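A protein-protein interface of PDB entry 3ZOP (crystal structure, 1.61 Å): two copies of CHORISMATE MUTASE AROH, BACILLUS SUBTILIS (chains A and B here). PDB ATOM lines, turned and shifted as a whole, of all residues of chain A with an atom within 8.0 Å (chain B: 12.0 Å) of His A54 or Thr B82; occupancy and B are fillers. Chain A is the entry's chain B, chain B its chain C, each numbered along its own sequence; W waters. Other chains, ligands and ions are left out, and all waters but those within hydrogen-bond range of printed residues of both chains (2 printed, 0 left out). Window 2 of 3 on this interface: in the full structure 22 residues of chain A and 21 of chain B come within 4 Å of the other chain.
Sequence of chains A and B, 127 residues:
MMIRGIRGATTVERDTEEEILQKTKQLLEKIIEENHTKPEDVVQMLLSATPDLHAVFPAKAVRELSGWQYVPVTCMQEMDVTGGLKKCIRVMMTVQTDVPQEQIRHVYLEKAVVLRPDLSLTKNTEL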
ATOM      1  N   ARG A  14       7.715  -4.491 -13.701  1.00  0.00           N
ATOM      2  CA  ARG A  14       7.411  -4.378 -12.282  1.00  0.00           C
ATOM      3  C   ARG A  14       7.347  -2.924 -11.820  1.00  0.00           C
ATOM      4  O   ARG A  14       7.948  -2.039 -12.426  1.00  0.00           O
ATOM      5  CB  ARG A  14       8.426  -5.156 -11.436  1.00  0.00           C
ATOM      6  CG  ARG A  14       9.869  -4.782 -11.664  1.00  0.00           C
ATOM      7  CD  ARG A  14      10.776  -5.650 -10.805  1.00  0.00           C
ATOM      8  NE  ARG A  14      10.163  -6.951 -10.576  1.00  0.00           N
ATOM      9  CZ  ARG A  14      10.194  -7.966 -11.433  1.00  0.00           C
ATOM     10  NH1 ARG A  14      10.815  -7.847 -12.606  1.00  0.00           N
ATOM     11  NH2 ARG A  14       9.594  -9.104 -11.117  1.00  0.00           N
ATOM     12  N   ASP A  15       6.605  -2.711 -10.740  1.00  0.00           N
ATOM     13  CA  ASP A  15       6.371  -1.380 -10.177  1.00  0.00           C
ATOM     14  C   ASP A  15       7.525  -0.937  -9.267  1.00  0.00           C
ATOM     15  O   ASP A  15       7.428  -0.969  -8.038  1.00  0.00           O
ATOM     16  CB  ASP A  15       5.033  -1.354  -9.436  1.00  0.00           C
ATOM     17  CG  ASP A  15       4.725   0.005  -8.837  1.00  0.00           C
ATOM     18  OD1 ASP A  15       5.259   1.013  -9.354  1.00  0.00           O
ATOM     19  OD2 ASP A  15       3.951   0.054  -7.859  1.00  0.00           O
ATOM     20  N   THR A  16       8.618  -0.519  -9.889  1.00  0.00           N
ATOM     21  CA  THR A  16       9.801  -0.073  -9.170  1.00  0.00           C
ATOM     22  C   THR A  16      10.296   1.210  -9.775  1.00  0.00           C
ATOM     23  O   THR A  16      10.087   1.478 -10.958  1.00  0.00           O
ATOM     24  CB  THR A  16      10.955  -1.110  -9.217  1.00  0.00           C
ATOM     25  OG1 THR A  16      11.426  -1.282 -10.571  1.00  0.00           O
ATOM     26  CG2 THR A  16      10.477  -2.444  -8.670  1.00  0.00           C
ATOM     27  N   GLU A  17      10.973   1.998  -8.961  1.00  0.00           N
ATOM     28  CA  GLU A  17      11.492   3.262  -9.419  1.00  0.00           C
ATOM     29  C   GLU A  17      12.474   3.075 -10.579  1.00  0.00           C
ATOM     30  O   GLU A  17      12.398   3.783 -11.580  1.00  0.00           O
ATOM     31  CB  GLU A  17      12.143   3.994  -8.255  1.00  0.00           C
ATOM     32  CG  GLU A  17      12.718   5.331  -8.604  1.00  0.00           C
ATOM     33  CD  GLU A  17      13.024   6.131  -7.366  1.00  0.00           C
ATOM     34  OE1 GLU A  17      12.607   5.700  -6.272  1.00  0.00           O
ATOM     35  OE2 GLU A  17      13.668   7.188  -7.481  1.00  0.00           O
ATOM     36  N   ILE A  20      10.419   2.209 -13.773  1.00  0.00           N
ATOM     37  CA  ILE A  20       9.621   3.332 -14.258  1.00  0.00           C
ATOM     38  C   ILE A  20      10.498   4.423 -14.856  1.00  0.00           C
ATOM     39  O   ILE A  20      10.221   4.930 -15.951  1.00  0.00           O
ATOM     40  CB  ILE A  20       8.735   3.910 -13.150  1.00  0.00           C
ATOM     41  CG1 ILE A  20       7.690   2.873 -12.749  1.00  0.00           C
ATOM     42  CG2 ILE A  20       8.044   5.184 -13.615  1.00  0.00           C
ATOM     43  CD1 ILE A  20       6.881   3.256 -11.525  1.00  0.00           C
ATOM     44  N   ALA A  49      -0.074   6.875 -16.085  1.00  0.00           N
ATOM     45  CA  ALA A  49       0.253   5.504 -15.674  1.00  0.00           C
ATOM     46  C   ALA A  49      -1.015   4.757 -15.299  1.00  0.00           C
ATOM     47  O   ALA A  49      -1.939   5.326 -14.718  1.00  0.00           O
ATOM     48  CB  ALA A  49       1.218   5.507 -14.501  1.00  0.00           C
ATOM     49  N   THR A  50      -1.072   3.477 -15.641  1.00  0.00           N
ATOM     50  CA  THR A  50      -2.167   2.652 -15.198  1.00  0.00           C
ATOM     51  C   THR A  50      -2.117   2.559 -13.687  1.00  0.00           C
ATOM     52  O   THR A  50      -1.069   2.791 -13.068  1.00  0.00           O
ATOM     53  CB  THR A  50      -2.082   1.252 -15.820  1.00  0.00           C
ATOM     54  OG1 THR A  50      -0.703   0.841 -15.848  1.00  0.00           O
ATOM     55  CG2 THR A  50      -2.610   1.284 -17.248  1.00  0.00           C
ATOM     56  N   PRO A  51      -3.264   2.241 -13.081  1.00  0.00           N
ATOM     57  CA  PRO A  51      -3.408   2.318 -11.630  1.00  0.00           C
ATOM     58  C   PRO A  51      -2.737   1.166 -10.880  1.00  0.00           C
ATOM     59  O   PRO A  51      -2.920   1.032  -9.660  1.00  0.00           O
ATOM     60  CB  PRO A  51      -4.924   2.302 -11.429  1.00  0.00           C
ATOM     61  CG  PRO A  51      -5.466   1.665 -12.671  1.00  0.00           C
ATOM     62  CD  PRO A  51      -4.550   2.034 -13.765  1.00  0.00           C
ATOM     63  N   ASP A  52      -1.942   0.367 -11.589  1.00  0.00           N
ATOM     64  CA  ASP A  52      -1.097  -0.647 -10.954  1.00  0.00           C
ATOM     65  C   ASP A  52       0.342  -0.167 -10.696  1.00  0.00           C
ATOM     66  O   ASP A  52       1.164  -0.910 -10.129  1.00  0.00           O
ATOM     67  CB  ASP A  52      -1.107  -1.949 -11.765  1.00  0.00           C
ATOM     68  CG  ASP A  52      -0.863  -1.718 -13.249  1.00  0.00           C
ATOM     69  OD1 ASP A  52      -0.499  -0.587 -13.640  1.00  0.00           O
ATOM     70  OD2 ASP A  52      -1.055  -2.669 -14.030  1.00  0.00           O
ATOM     71  N   LEU A  53       0.636   1.078 -11.074  1.00  0.00           N
ATOM     72  CA  LEU A  53       1.969   1.663 -10.865  1.00  0.00           C
ATOM     73  C   LEU A  53       1.946   2.788  -9.844  1.00  0.00           C
ATOM     74  O   LEU A  53       1.173   3.743  -9.994  1.00  0.00           O
ATOM     75  CB  LEU A  53       2.538   2.202 -12.176  1.00  0.00           C
ATOM     76  CG  LEU A  53       2.710   1.142 -13.268  1.00  0.00           C
ATOM     77  CD1 LEU A  53       3.282   1.794 -14.523  1.00  0.00           C
ATOM     78  CD2 LEU A  53       3.612   0.005 -12.805  1.00  0.00           C
ATOM     79  N   HIS A  54       2.807   2.697  -8.829  1.00  0.00           N
ATOM     80  CA  HIS A  54       2.784   3.677  -7.731  1.00  0.00           C
ATOM     81  C   HIS A  54       4.160   4.075  -7.231  1.00  0.00           C
ATOM     82  O   HIS A  54       4.269   4.940  -6.360  1.00  0.00           O
ATOM     83  CB  HIS A  54       2.019   3.109  -6.544  1.00  0.00           C
ATOM     84  CG  HIS A  54       0.650   2.629  -6.895  1.00  0.00           C
ATOM     85  ND1 HIS A  54      -0.410   3.488  -7.092  1.00  0.00           N
ATOM     86  CD2 HIS A  54       0.174   1.381  -7.108  1.00  0.00           C
ATOM     87  CE1 HIS A  54      -1.486   2.786  -7.403  1.00  0.00           C
ATOM     88  NE2 HIS A  54      -1.157   1.507  -7.422  1.00  0.00           N
ATOM     89  N   ALA A  55       5.213   3.442  -7.736  1.00  0.00           N
ATOM     90  CA  ALA A  55       6.507   3.604  -7.085  1.00  0.00           C
ATOM     91  C   ALA A  55       7.106   5.007  -7.174  1.00  0.00           C
ATOM     92  O   ALA A  55       7.775   5.455  -6.242  1.00  0.00           O
ATOM     93  CB  ALA A  55       7.505   2.574  -7.595  1.00  0.00           C
ATOM     94  N   VAL A  56       6.903   5.681  -8.303  1.00  0.00           N
ATOM     95  CA  VAL A  56       7.500   6.998  -8.540  1.00  0.00           C
ATOM     96  C   VAL A  56       6.730   7.711  -9.652  1.00  0.00           C
ATOM     97  O   VAL A  56       6.096   7.048 -10.472  1.00  0.00           O
ATOM     98  CB  VAL A  56       8.979   6.847  -8.978  1.00  0.00           C
ATOM     99  CG1 VAL A  56       9.076   6.176 -10.351  1.00  0.00           C
ATOM    100  CG2 VAL A  56       9.690   8.198  -8.990  1.00  0.00           C
ATOM    101  N   PHE A  57       6.752   9.045  -9.669  1.00  0.00           N
ATOM    102  CA  PHE A  57       6.198   9.781 -10.809  1.00  0.00           C
ATOM    103  C   PHE A  57       7.094   9.620 -12.030  1.00  0.00           C
ATOM    104  O   PHE A  57       8.281   9.896 -11.945  1.00  0.00           O
ATOM    105  CB  PHE A  57       6.094  11.288 -10.515  1.00  0.00           C
ATOM    106  CG  PHE A  57       4.995  11.664  -9.561  1.00  0.00           C
ATOM    107  CD1 PHE A  57       3.670  11.589  -9.947  1.00  0.00           C
ATOM    108  CD2 PHE A  57       5.291  12.104  -8.282  1.00  0.00           C
ATOM    109  CE1 PHE A  57       2.651  11.938  -9.096  1.00  0.00           C
ATOM    110  CE2 PHE A  57       4.272  12.457  -7.407  1.00  0.00           C
ATOM    111  CZ  PHE A  57       2.947  12.378  -7.819  1.00  0.00           C
ATOM    112  N   PRO A  58       6.528   9.198 -13.178  1.00  0.00           N
ATOM    113  CA  PRO A  58       7.364   9.081 -14.386  1.00  0.00           C
ATOM    114  C   PRO A  58       8.023  10.412 -14.772  1.00  0.00           C
ATOM    115  O   PRO A  58       9.074  10.424 -15.415  1.00  0.00           O
ATOM    116  CB  PRO A  58       6.373   8.640 -15.468  1.00  0.00           C
ATOM    117  CG  PRO A  58       5.230   8.031 -14.752  1.00  0.00           C
ATOM    118  CD  PRO A  58       5.167   8.679 -13.382  1.00  0.00           C
ATOM    119  N   GLN A  77      -3.586   9.605 -13.747  1.00  0.00           N
ATOM    120  CA  GLN A  77      -3.935   8.188 -13.760  1.00  0.00           C
ATOM    121  C   GLN A  77      -4.672   7.851 -15.055  1.00  0.00           C
ATOM    122  O   GLN A  77      -5.647   8.517 -15.413  1.00  0.00           O
ATOM    123  CB  GLN A  77      -4.781   7.849 -12.526  1.00  0.00           C
ATOM    124  CG  GLN A  77      -5.121   6.369 -12.352  1.00  0.00           C
ATOM    125  CD  GLN A  77      -5.631   6.048 -10.962  1.00  0.00           C
ATOM    126  OE1 GLN A  77      -4.902   6.177  -9.979  1.00  0.00           O
ATOM    127  NE2 GLN A  77      -6.879   5.607 -10.873  1.00  0.00           N
ATOM    128  N   ALA B  49      -6.204  16.330  -8.850  1.00  0.00           N
ATOM    129  CA  ALA B  49      -6.188  16.193  -7.397  1.00  0.00           C
ATOM    130  C   ALA B  49      -5.701  14.816  -7.040  1.00  0.00           C
ATOM    131  O   ALA B  49      -5.966  13.852  -7.756  1.00  0.00           O
ATOM    132  CB  ALA B  49      -7.585  16.422  -6.817  1.00  0.00           C
ATOM    133  N   THR B  50      -4.994  14.707  -5.926  1.00  0.00           N
ATOM    134  CA  THR B  50      -4.657  13.386  -5.412  1.00  0.00           C
ATOM    135  C   THR B  50      -5.947  12.668  -4.996  1.00  0.00           C
ATOM    136  O   THR B  50      -6.960  13.314  -4.709  1.00  0.00           O
ATOM    137  CB  THR B  50      -3.648  13.490  -4.266  1.00  0.00           C
ATOM    138  OG1 THR B  50      -4.071  14.525  -3.369  1.00  0.00           O
ATOM    139  CG2 THR B  50      -2.258  13.859  -4.846  1.00  0.00           C
ATOM    140  N   PRO B  51      -5.912  11.334  -4.945  1.00  0.00           N
ATOM    141  CA  PRO B  51      -7.157  10.586  -4.718  1.00  0.00           C
ATOM    142  C   PRO B  51      -7.674  10.596  -3.290  1.00  0.00           C
ATOM    143  O   PRO B  51      -8.618   9.851  -2.959  1.00  0.00           O
ATOM    144  CB  PRO B  51      -6.795   9.163  -5.175  1.00  0.00           C
ATOM    145  CG  PRO B  51      -5.309   9.094  -5.037  1.00  0.00           C
ATOM    146  CD  PRO B  51      -4.796  10.461  -5.348  1.00  0.00           C
ATOM    147  N   ASP B  52      -7.095  11.453  -2.454  1.00  0.00           N
ATOM    148  CA  ASP B  52      -7.633  11.710  -1.113  1.00  0.00           C
ATOM    149  C   ASP B  52      -8.498  12.976  -1.047  1.00  0.00           C
ATOM    150  O   ASP B  52      -8.921  13.408   0.053  1.00  0.00           O
ATOM    151  CB  ASP B  52      -6.491  11.790  -0.094  1.00  0.00           C
ATOM    152  CG  ASP B  52      -5.394  12.763  -0.510  1.00  0.00           C
ATOM    153  OD1 ASP B  52      -5.576  13.475  -1.513  1.00  0.00           O
ATOM    154  OD2 ASP B  52      -4.341  12.819   0.165  1.00  0.00           O
ATOM    155  N   GLN B  77      -7.591  12.812 -12.135  1.00  0.00           N
ATOM    156  CA  GLN B  77      -6.972  12.266 -10.947  1.00  0.00           C
ATOM    157  C   GLN B  77      -5.469  12.198 -11.139  1.00  0.00           C
ATOM    158  O   GLN B  77      -4.976  11.641 -12.122  1.00  0.00           O
ATOM    159  CB  GLN B  77      -7.511  10.865 -10.662  1.00  0.00           C
ATOM    160  CG  GLN B  77      -7.437  10.456  -9.202  1.00  0.00           C
ATOM    161  CD  GLN B  77      -8.569  11.102  -8.389  1.00  0.00           C
ATOM    162  OE1 GLN B  77      -9.742  10.717  -8.495  1.00  0.00           O
ATOM    163  NE2 GLN B  77      -8.219  12.104  -7.593  1.00  0.00           N
ATOM    164  N   GLU B  78      -4.739  12.770 -10.197  1.00  0.00           N
ATOM    165  CA  GLU B  78      -3.305  12.623 -10.161  1.00  0.00           C
ATOM    166  C   GLU B  78      -2.923  11.172  -9.909  1.00  0.00           C
ATOM    167  O   GLU B  78      -3.629  10.428  -9.238  1.00  0.00           O
ATOM    168  CB  GLU B  78      -2.746  13.508  -9.047  1.00  0.00           C
ATOM    169  CG  GLU B  78      -1.289  13.241  -8.794  1.00  0.00           C
ATOM    170  CD  GLU B  78      -0.480  14.491  -8.730  1.00  0.00           C
ATOM    171  OE1 GLU B  78      -0.732  15.332  -7.813  1.00  0.00           O
ATOM    172  OE2 GLU B  78       0.406  14.623  -9.612  1.00  0.00           O
ATOM    173  N   MET B  79      -1.793  10.761 -10.464  1.00  0.00           N
ATOM    174  CA  MET B  79      -1.254   9.464 -10.170  1.00  0.00           C
ATOM    175  C   MET B  79      -1.053   9.313  -8.659  1.00  0.00           C
ATOM    176  O   MET B  79      -0.640  10.258  -7.969  1.00  0.00           O
ATOM    177  CB  MET B  79       0.063   9.333 -10.919  1.00  0.00           C
ATOM    178  CG  MET B  79       0.730   8.015 -10.782  1.00  0.00           C
ATOM    179  SD  MET B  79       2.260   8.045 -11.707  1.00  0.00           S
ATOM    180  CE  MET B  79       2.855   6.404 -11.294  1.00  0.00           C
ATOM    181  N   ASP B  80      -1.390   8.139  -8.140  1.00  0.00           N
ATOM    182  CA  ASP B  80      -1.243   7.832  -6.727  1.00  0.00           C
ATOM    183  C   ASP B  80       0.151   7.251  -6.493  1.00  0.00           C
ATOM    184  O   ASP B  80       0.396   6.088  -6.806  1.00  0.00           O
ATOM    185  CB  ASP B  80      -2.317   6.820  -6.342  1.00  0.00           C
ATOM    186  CG  ASP B  80      -2.386   6.553  -4.857  1.00  0.00           C
ATOM    187  OD1 ASP B  80      -1.673   7.216  -4.073  1.00  0.00           O
ATOM    188  OD2 ASP B  80      -3.190   5.671  -4.479  1.00  0.00           O
ATOM    189  N   VAL B  81       1.068   8.064  -5.974  1.00  0.00           N
ATOM    190  CA  VAL B  81       2.453   7.632  -5.795  1.00  0.00           C
ATOM    191  C   VAL B  81       2.691   7.339  -4.326  1.00  0.00           C
ATOM    192  O   VAL B  81       2.308   8.125  -3.457  1.00  0.00           O
ATOM    193  CB  VAL B  81       3.443   8.691  -6.312  1.00  0.00           C
ATOM    194  CG1 VAL B  81       4.864   8.402  -5.843  1.00  0.00           C
ATOM    195  CG2 VAL B  81       3.374   8.756  -7.830  1.00  0.00           C
ATOM    196  N   THR B  82       3.266   6.173  -4.056  1.00  0.00           N
ATOM    197  CA  THR B  82       3.633   5.753  -2.720  1.00  0.00           C
ATOM    198  C   THR B  82       4.546   6.780  -2.069  1.00  0.00           C
ATOM    199  O   THR B  82       5.621   7.085  -2.585  1.00  0.00           O
ATOM    200  CB  THR B  82       4.366   4.409  -2.803  1.00  0.00           C
ATOM    201  OG1 THR B  82       3.577   3.504  -3.583  1.00  0.00           O
ATOM    202  CG2 THR B  82       4.627   3.832  -1.419  1.00  0.00           C
ATOM    203  N   GLY B  83       4.107   7.312  -0.937  1.00  0.00           N
ATOM    204  CA  GLY B  83       4.872   8.325  -0.229  1.00  0.00           C
ATOM    205  C   GLY B  83       4.804   9.701  -0.871  1.00  0.00           C
ATOM    206  O   GLY B  83       5.532  10.614  -0.460  1.00  0.00           O
ATOM    207  N   GLY B  84       3.942   9.859  -1.877  1.00  0.00           N
ATOM    208  CA  GLY B  84       3.765  11.157  -2.546  1.00  0.00           C
ATOM    209  C   GLY B  84       3.083  12.194  -1.658  1.00  0.00           C
ATOM    210  O   GLY B  84       2.494  11.862  -0.632  1.00  0.00           O
ATOM    211  N   LEU B  85       3.166  13.456  -2.050  1.00  0.00           N
ATOM    212  CA  LEU B  85       2.566  14.517  -1.259  1.00  0.00           C
ATOM    213  C   LEU B  85       1.057  14.323  -1.222  1.00  0.00           C
ATOM    214  O   LEU B  85       0.419  14.113  -2.254  1.00  0.00           O
ATOM    215  CB  LEU B  85       2.901  15.870  -1.888  1.00  0.00           C
ATOM    216  CG  LEU B  85       2.412  17.148  -1.244  1.00  0.00           C
ATOM    217  CD1 LEU B  85       3.024  17.313   0.135  1.00  0.00           C
ATOM    218  CD2 LEU B  85       2.798  18.306  -2.134  1.00  0.00           C
ATOM    219  N   LYS B  86       0.467  14.404  -0.040  1.00  0.00           N
ATOM    220  CA  LYS B  86      -0.968  14.189   0.075  1.00  0.00           C
ATOM    221  C   LYS B  86      -1.762  15.483  -0.106  1.00  0.00           C
ATOM    222  O   LYS B  86      -1.202  16.581  -0.025  1.00  0.00           O
ATOM    223  CB  LYS B  86      -1.294  13.574   1.428  1.00  0.00           C
ATOM    224  CG  LYS B  86      -0.585  12.272   1.723  1.00  0.00           C
ATOM    225  CD  LYS B  86      -0.958  11.172   0.725  1.00  0.00           C
ATOM    226  CE  LYS B  86      -0.142   9.889   0.987  1.00  0.00           C
ATOM    227  NZ  LYS B  86       0.184   9.174  -0.276  1.00  0.00           N
ATOM    228  N   LYS B  87      -3.065  15.343  -0.362  1.00  0.00           N
ATOM    229  CA  LYS B  87      -3.986  16.485  -0.397  1.00  0.00           C
ATOM    230  C   LYS B  87      -3.474  17.575  -1.336  1.00  0.00           C
ATOM    231  O   LYS B  87      -3.453  18.762  -1.003  1.00  0.00           O
ATOM    232  CB  LYS B  87      -4.236  17.044   1.024  1.00  0.00           C
ATOM    233  CG  LYS B  87      -5.046  16.077   1.884  1.00  0.00           C
ATOM    234  CD  LYS B  87      -5.356  16.662   3.274  1.00  0.00           C
ATOM    235  CE  LYS B  87      -5.998  15.620   4.171  1.00  0.00           C
ATOM    236  NZ  LYS B  87      -5.113  14.434   4.315  1.00  0.00           N
ATOM    237  C   CIR B  90      -2.804  21.433 -10.584  1.00  0.00           C
ATOM    238  O   CIR B  90      -3.955  21.042 -10.902  1.00  0.00           O
ATOM    239  CA  CIR B  90      -2.050  20.754  -9.473  1.00  0.00           C
ATOM    240  N   CIR B  90      -2.990  20.235  -8.492  1.00  0.00           N
ATOM    241  C3  CIR B  90      -1.188  19.606 -10.011  1.00  0.00           C
ATOM    242  C4  CIR B  90      -0.278  19.080  -8.902  1.00  0.00           C
ATOM    243  C5  CIR B  90       0.602  17.893  -9.288  1.00  0.00           C
ATOM    244  N6  CIR B  90       1.273  17.439  -8.072  1.00  0.00           N
ATOM    245  C7  CIR B  90       2.355  16.666  -7.933  1.00  0.00           C
ATOM    246  O7  CIR B  90       3.292  16.687  -8.726  1.00  0.00           O
ATOM    247  N8  CIR B  90       2.400  15.870  -6.852  1.00  0.00           N
ATOM    248  N   LEU B 115       7.801  20.504  -4.144  1.00  0.00           N
ATOM    249  CA  LEU B 115       7.783  20.003  -5.512  1.00  0.00           C
ATOM    250  C   LEU B 115       8.576  20.899  -6.466  1.00  0.00           C
ATOM    251  O   LEU B 115       8.773  20.554  -7.635  1.00  0.00           O
ATOM    252  CB  LEU B 115       6.348  19.845  -6.005  1.00  0.00           C
ATOM    253  CG  LEU B 115       5.425  18.961  -5.167  1.00  0.00           C
ATOM    254  CD1 LEU B 115       4.025  18.986  -5.759  1.00  0.00           C
ATOM    255  CD2 LEU B 115       5.934  17.533  -5.053  1.00  0.00           C
HETATM  256  O   HOH W   1       4.775   1.277  -5.166  1.00  0.00           O
HETATM  257  O   HOH W   2      -2.278   5.787  -9.475  1.00  0.00           O
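O of Ala B49 lies within hydrogen-bond range of N of Glu B78.
N of His A54 lies within hydrogen-bond range of OD1 of Asp A15, 3.0 Å away.
NE2 of Gln B77 lies within hydrogen-bond range of O of Thr B50, at 3.4 Å.
N6 of CIR B90 is in hydrogen-bond range of the side-chain carboxylate of Glu B78 (2.9 Å).
The backbone carbonyl oxygen of Ala B49 lies within hydrogen-bond range of the side-chain amide nitrogen of Gln B77 (2.9 Å).
A ring nitrogen (NE2) of His A54 lies within hydrogen-bond range of the backbone carbonyl oxygen of Pro A51 (2.9 Å).
Hydrophobic or aromatic side chains of chain B that line the printed part of chain A: Met B79 and Val B81.
Along chain B the printed residues that touch a printed residue of chain A span positions 77 to 90.
Among the printed residues, 14 pairs touch across the chains.
Among the printed residues, no Asp or Glu carboxylate lies within 4 Å of a Lys or Arg side-chain nitrogen of the other chain.
Water W2 lies within hydrogen-bond range of OE1 of Gln A77 (2.7 Å) and N of Asp B80 (2.8 Å).
Water W1 lies within hydrogen-bond range of OG1 of Thr B82 (3.0 Å), OD2 of Asp A15 (3.1 Å) and N of Ala A55 (3.4 Å).
Of the printed residues of chain B, His A54 touches Asp B80, Val B81 and Thr B82.
Thr B82 touches just one residue of chain A: His A54 (2.8 Å).
No residue of chain B comes within 4 Å of Pro A51.
No residue of chain B comes within 4 Å of Asp A52.
Leu A53 touches just one residue of chain B: Met B79.
No residue of chain B comes within 4 Å of Ala A55.
Val A56 touches just these residues of chain B: Met B79 (3.4 Å) and Val B81 (3.96 Å).
Of the printed residues of chain B, Ala A49 touches Met B79.
Of the printed residues of chain B, Gln A77 touches Gln B77 (3.0 Å) and Met B79 (3.9 Å).
Printed residues of chain A within 4 Å of Asp B80: His A54.
Printed residues of chain B within 4 Å of Pro A58: Met B79 (3.4 Å).
Leu B85 touches none of the printed residues of chain A.
The nearest residue of chain B that does not touch His A54 is Met B79 (4.5 Å).
The backbone NH (N) of Thr B82 lies within hydrogen-bond range of the backbone carbonyl oxygen (O) of His A54 (2.8 Å).
The backbone carbonyl oxygen (O) of Gln B77 lies within hydrogen-bond range of the backbone NH (N) of Gln A77, at 3.0 Å.
A ring nitrogen (ND1) of His A54 is in hydrogen-bond range of the backbone carbonyl oxygen (O) of Asp B80 (2.7 Å).
Gln A77 touches its own counterpart, Gln B77.
Positions printed for both chains: 49, 50, 51, 52 and 77.
Of the 14 pairs that touch across the chains among the printed residues, 1 has its exchanged pair printed and touching as well.
Among the printed residues, merely in contact across the chains: His A54 with Val B81, Val A56 with Met B79, Leu A53 with Met B79, Pro A58 with Met B79, Phe A57 with Val B81, Phe A57 with Glu B78, Phe A57 with CIR B90, Ala A49 with Met B79, Phe A57 with Met B79, Gln A77 with Met B79 and Val A56 with Val B81.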
